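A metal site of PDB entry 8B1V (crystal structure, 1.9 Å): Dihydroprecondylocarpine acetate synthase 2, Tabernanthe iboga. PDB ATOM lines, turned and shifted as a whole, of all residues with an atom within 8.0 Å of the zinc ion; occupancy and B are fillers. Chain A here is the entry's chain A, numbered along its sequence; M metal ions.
OG1 of Thr 104 sits close to SG of Cys 111, at 3.1 Å.
The side-chain sulfur (SG) of Cys 108 sits close to the backbone NH (N) of Asn 110, at 3.6 Å.
SG of Cys 119 sits close to N of Glu 121 (3.3 Å).
The backbone carbonyl oxygen (O) of Cys 111 lies within hydrogen-bond range of the guanidinium group (NH2) of Arg 149, at 2.8 Å.
The side-chain sulfur of Cys 111 lies close to the backbone NH of Gly 106 (3.2 Å).
The side-chain sulfur of Cys 105 lies close to the backbone NH of Lys 107 (3.2 Å).
N of Gly 106 touches the zinc ion, 3.8 Å away.
Of the 19 residues printed, 5 come within 4 Å of the zinc ion.
Along chain A the residues within 4 Å of the zinc ion span positions 105 to 119.
The nearest printed residue that does not touch the zinc ion is Lys 107 (4.4 Å).
The zinc ion is bound by the side-chain sulfur of Cys 108 (2.3 Å), the side-chain sulfur of Cys 105 (2.3 Å), the side-chain sulfur of Cys 111 (2.3 Å) and the side-chain sulfur of Cys 119 (2.3 Å).
The zinc ion has four donor atoms within binding distance.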
ATOM      1  N   GLY A 103      22.502 -12.155 -21.853  1.00  0.00           N
ATOM      2  CA  GLY A 103      23.622 -12.423 -20.982  1.00  0.00           C
ATOM      3  C   GLY A 103      24.844 -11.636 -21.406  1.00  0.00           C
ATOM      4  O   GLY A 103      24.913 -11.121 -22.533  1.00  0.00           O
ATOM      5  N   THR A 104      25.795 -11.546 -20.484  1.00  0.00           N
ATOM      6  CA  THR A 104      27.061 -10.841 -20.686  1.00  0.00           C
ATOM      7  C   THR A 104      28.173 -11.598 -19.965  1.00  0.00           C
ATOM      8  O   THR A 104      27.917 -12.571 -19.240  1.00  0.00           O
ATOM      9  CB  THR A 104      26.988  -9.384 -20.194  1.00  0.00           C
ATOM     10  OG1 THR A 104      26.858  -9.352 -18.765  1.00  0.00           O
ATOM     11  CG2 THR A 104      25.836  -8.606 -20.835  1.00  0.00           C
ATOM     12  N   CYS A 105      29.415 -11.164 -20.186  1.00  0.00           N
ATOM     13  CA  CYS A 105      30.547 -11.874 -19.575  1.00  0.00           C
ATOM     14  C   CYS A 105      30.556 -11.755 -18.057  1.00  0.00           C
ATOM     15  O   CYS A 105      31.013 -12.681 -17.373  1.00  0.00           O
ATOM     16  CB  CYS A 105      31.878 -11.375 -20.157  1.00  0.00           C
ATOM     17  SG  CYS A 105      32.561  -9.865 -19.413  1.00  0.00           S
ATOM     18  N   GLY A 106      30.055 -10.648 -17.515  1.00  0.00           N
ATOM     19  CA  GLY A 106      30.027 -10.440 -16.081  1.00  0.00           C
ATOM     20  C   GLY A 106      31.306  -9.911 -15.455  1.00  0.00           C
ATOM     21  O   GLY A 106      31.278  -9.531 -14.275  1.00  0.00           O
ATOM     22  N   LYS A 107      32.415  -9.852 -16.194  1.00  0.00           N
ATOM     23  CA  LYS A 107      33.706  -9.480 -15.641  1.00  0.00           C
ATOM     24  C   LYS A 107      34.271  -8.161 -16.147  1.00  0.00           C
ATOM     25  O   LYS A 107      35.019  -7.497 -15.415  1.00  0.00           O
ATOM     26  CB  LYS A 107      34.744 -10.583 -15.914  1.00  0.00           C
ATOM     27  CG  LYS A 107      34.226 -11.992 -15.686  1.00  0.00           C
ATOM     28  N   CYS A 108      33.956  -7.760 -17.376  1.00  0.00           N
ATOM     29  CA  CYS A 108      34.566  -6.588 -17.971  1.00  0.00           C
ATOM     30  C   CYS A 108      34.074  -5.302 -17.301  1.00  0.00           C
ATOM     31  O   CYS A 108      33.189  -5.317 -16.446  1.00  0.00           O
ATOM     32  CB  CYS A 108      34.284  -6.556 -19.484  1.00  0.00           C
ATOM     33  SG  CYS A 108      32.576  -6.127 -19.918  1.00  0.00           S
ATOM     34  N   TYR A 109      34.682  -4.182 -17.696  1.00  0.00           N
ATOM     35  CA  TYR A 109      34.326  -2.877 -17.138  1.00  0.00           C
ATOM     36  C   TYR A 109      32.834  -2.593 -17.314  1.00  0.00           C
ATOM     37  O   TYR A 109      32.173  -2.097 -16.390  1.00  0.00           O
ATOM     38  CB  TYR A 109      35.151  -1.779 -17.803  1.00  0.00           C
ATOM     39  CG  TYR A 109      34.925  -0.397 -17.207  1.00  0.00           C
ATOM     40  CD1 TYR A 109      35.619   0.021 -16.086  1.00  0.00           C
ATOM     41  CD2 TYR A 109      33.970   0.452 -17.754  1.00  0.00           C
ATOM     42  CE1 TYR A 109      35.409   1.276 -15.542  1.00  0.00           C
ATOM     43  CE2 TYR A 109      33.738   1.701 -17.206  1.00  0.00           C
ATOM     44  CZ  TYR A 109      34.463   2.115 -16.107  1.00  0.00           C
ATOM     45  OH  TYR A 109      34.232   3.356 -15.578  1.00  0.00           O
ATOM     46  N   ASN A 110      32.313  -2.858 -18.509  1.00  0.00           N
ATOM     47  CA  ASN A 110      30.907  -2.554 -18.785  1.00  0.00           C
ATOM     48  C   ASN A 110      29.974  -3.332 -17.867  1.00  0.00           C
ATOM     49  O   ASN A 110      29.009  -2.779 -17.322  1.00  0.00           O
ATOM     50  CB  ASN A 110      30.601  -2.853 -20.256  1.00  0.00           C
ATOM     51  CG  ASN A 110      31.520  -2.118 -21.199  1.00  0.00           C
ATOM     52  OD1 ASN A 110      31.526  -0.886 -21.244  1.00  0.00           O
ATOM     53  ND2 ASN A 110      32.315  -2.866 -21.957  1.00  0.00           N
ATOM     54  N   CYS A 111      30.238  -4.630 -17.689  1.00  0.00           N
ATOM     55  CA  CYS A 111      29.372  -5.450 -16.841  1.00  0.00           C
ATOM     56  C   CYS A 111      29.426  -4.991 -15.392  1.00  0.00           C
ATOM     57  O   CYS A 111      28.375  -4.852 -14.734  1.00  0.00           O
ATOM     58  CB  CYS A 111      29.784  -6.922 -16.951  1.00  0.00           C
ATOM     59  SG  CYS A 111      29.479  -7.646 -18.570  1.00  0.00           S
ATOM     60  N   VAL A 112      30.631  -4.755 -14.873  1.00  0.00           N
ATOM     61  CA  VAL A 112      30.816  -4.465 -13.460  1.00  0.00           C
ATOM     62  C   VAL A 112      30.261  -3.102 -13.077  1.00  0.00           C
ATOM     63  O   VAL A 112      29.881  -2.880 -11.914  1.00  0.00           O
ATOM     64  CB  VAL A 112      32.320  -4.613 -13.126  1.00  0.00           C
ATOM     65  CG1 VAL A 112      32.730  -3.724 -11.960  1.00  0.00           C
ATOM     66  CG2 VAL A 112      32.652  -6.063 -12.848  1.00  0.00           C
ATOM     67  N   LEU A 115      26.831  -1.173 -17.269  1.00  0.00           N
ATOM     68  CA  LEU A 115      26.741  -0.701 -18.636  1.00  0.00           C
ATOM     69  C   LEU A 115      26.811  -1.888 -19.581  1.00  0.00           C
ATOM     70  O   LEU A 115      27.452  -1.853 -20.636  1.00  0.00           O
ATOM     71  CB  LEU A 115      27.873   0.283 -18.950  1.00  0.00           C
ATOM     72  CG  LEU A 115      28.012   1.513 -18.041  1.00  0.00           C
ATOM     73  CD1 LEU A 115      29.039   2.483 -18.610  1.00  0.00           C
ATOM     74  CD2 LEU A 115      26.672   2.203 -17.868  1.00  0.00           C
ATOM     75  N   GLU A 116      26.127  -2.971 -19.201  1.00  0.00           N
ATOM     76  CA  GLU A 116      26.450  -4.291 -19.729  1.00  0.00           C
ATOM     77  C   GLU A 116      25.919  -4.519 -21.138  1.00  0.00           C
ATOM     78  O   GLU A 116      26.351  -5.488 -21.786  1.00  0.00           O
ATOM     79  CB  GLU A 116      25.940  -5.380 -18.779  1.00  0.00           C
ATOM     80  CG  GLU A 116      24.431  -5.572 -18.694  1.00  0.00           C
ATOM     81  CD  GLU A 116      23.672  -4.359 -18.193  1.00  0.00           C
ATOM     82  OE1 GLU A 116      24.081  -3.749 -17.174  1.00  0.00           O
ATOM     83  OE2 GLU A 116      22.622  -4.033 -18.796  1.00  0.00           O
ATOM     84  N   ASN A 117      25.012  -3.679 -21.639  1.00  0.00           N
ATOM     85  CA  ASN A 117      24.628  -3.782 -23.044  1.00  0.00           C
ATOM     86  C   ASN A 117      25.812  -3.580 -23.982  1.00  0.00           C
ATOM     87  O   ASN A 117      25.759  -4.032 -25.126  1.00  0.00           O
ATOM     88  CB  ASN A 117      23.515  -2.782 -23.381  1.00  0.00           C
ATOM     89  CG  ASN A 117      23.912  -1.339 -23.115  1.00  0.00           C
ATOM     90  OD1 ASN A 117      24.485  -1.017 -22.068  1.00  0.00           O
ATOM     91  ND2 ASN A 117      23.608  -0.459 -24.068  1.00  0.00           N
ATOM     92  N   TYR A 118      26.887  -2.939 -23.512  1.00  0.00           N
ATOM     93  CA  TYR A 118      28.086  -2.740 -24.306  1.00  0.00           C
ATOM     94  C   TYR A 118      29.190  -3.731 -23.951  1.00  0.00           C
ATOM     95  O   TYR A 118      30.371  -3.476 -24.242  1.00  0.00           O
ATOM     96  CB  TYR A 118      28.577  -1.297 -24.152  1.00  0.00           C
ATOM     97  CG  TYR A 118      27.664  -0.314 -24.828  1.00  0.00           C
ATOM     98  CD1 TYR A 118      27.415  -0.372 -26.191  1.00  0.00           C
ATOM     99  CD2 TYR A 118      26.987   0.655 -24.086  1.00  0.00           C
ATOM    100  CE1 TYR A 118      26.558   0.516 -26.814  1.00  0.00           C
ATOM    101  CE2 TYR A 118      26.131   1.548 -24.700  1.00  0.00           C
ATOM    102  CZ  TYR A 118      25.921   1.475 -26.057  1.00  0.00           C
ATOM    103  OH  TYR A 118      25.053   2.356 -26.676  1.00  0.00           O
ATOM    104  N   CYS A 119      28.849  -4.839 -23.304  1.00  0.00           N
ATOM    105  CA  CYS A 119      29.794  -5.926 -23.110  1.00  0.00           C
ATOM    106  C   CYS A 119      30.241  -6.469 -24.469  1.00  0.00           C
ATOM    107  O   CYS A 119      29.396  -6.737 -25.335  1.00  0.00           O
ATOM    108  CB  CYS A 119      29.172  -7.056 -22.282  1.00  0.00           C
ATOM    109  SG  CYS A 119      30.242  -8.514 -22.086  1.00  0.00           S
ATOM    110  N   PRO A 120      31.545  -6.656 -24.694  1.00  0.00           N
ATOM    111  CA  PRO A 120      31.994  -7.238 -25.969  1.00  0.00           C
ATOM    112  C   PRO A 120      31.470  -8.639 -26.207  1.00  0.00           C
ATOM    113  O   PRO A 120      31.410  -9.075 -27.370  1.00  0.00           O
ATOM    114  CB  PRO A 120      33.523  -7.236 -25.858  1.00  0.00           C
ATOM    115  CG  PRO A 120      33.868  -6.384 -24.695  1.00  0.00           C
ATOM    116  CD  PRO A 120      32.655  -6.205 -23.831  1.00  0.00           C
ATOM    117  N   GLU A 121      31.084  -9.368 -25.161  1.00  0.00           N
ATOM    118  CA  GLU A 121      30.544 -10.712 -25.281  1.00  0.00           C
ATOM    119  C   GLU A 121      29.054 -10.772 -24.949  1.00  0.00           C
ATOM    120  O   GLU A 121      28.557 -11.796 -24.480  1.00  0.00           O
ATOM    121  CB  GLU A 121      31.332 -11.683 -24.399  1.00  0.00           C
ATOM    122  CG  GLU A 121      32.840 -11.515 -24.539  1.00  0.00           C
ATOM    123  CD  GLU A 121      33.581 -12.839 -24.561  1.00  0.00           C
ATOM    124  OE1 GLU A 121      33.127 -13.786 -23.864  1.00  0.00           O
ATOM    125  OE2 GLU A 121      34.608 -12.942 -25.267  1.00  0.00           O
ATOM    126  N   VAL A 122      28.334  -9.667 -25.180  1.00  0.00           N
ATOM    127  CA  VAL A 122      26.896  -9.653 -24.938  1.00  0.00           C
ATOM    128  C   VAL A 122      26.212 -10.722 -25.784  1.00  0.00           C
ATOM    129  O   VAL A 122      26.589 -10.966 -26.948  1.00  0.00           O
ATOM    130  CB  VAL A 122      26.337  -8.243 -25.203  1.00  0.00           C
ATOM    131  CG1 VAL A 122      26.479  -7.873 -26.672  1.00  0.00           C
ATOM    132  CG2 VAL A 122      24.861  -8.168 -24.768  1.00  0.00           C
ATOM    133  N   ARG A 149      18.977 -10.797 -13.988  1.00  0.00           N
ATOM    134  CA  ARG A 149      19.574  -9.495 -14.279  1.00  0.00           C
ATOM    135  C   ARG A 149      18.957  -8.854 -15.511  1.00  0.00           C
ATOM    136  O   ARG A 149      18.924  -7.623 -15.620  1.00  0.00           O
ATOM    137  CB  ARG A 149      21.096  -9.626 -14.459  1.00  0.00           C
ATOM    138  CG  ARG A 149      21.786  -8.272 -14.611  1.00  0.00           C
ATOM    139  CD  ARG A 149      23.297  -8.415 -14.796  1.00  0.00           C
ATOM    140  NE  ARG A 149      23.922  -7.103 -14.960  1.00  0.00           N
ATOM    141  CZ  ARG A 149      25.230  -6.900 -15.012  1.00  0.00           C
ATOM    142  NH1 ARG A 149      26.100  -7.896 -14.934  1.00  0.00           N
ATOM    143  NH2 ARG A 149      25.694  -5.655 -15.130  1.00  0.00           N
HETATM  144 ZN    ZN M   1      31.259  -8.036 -20.034  1.00  0.00          ZN
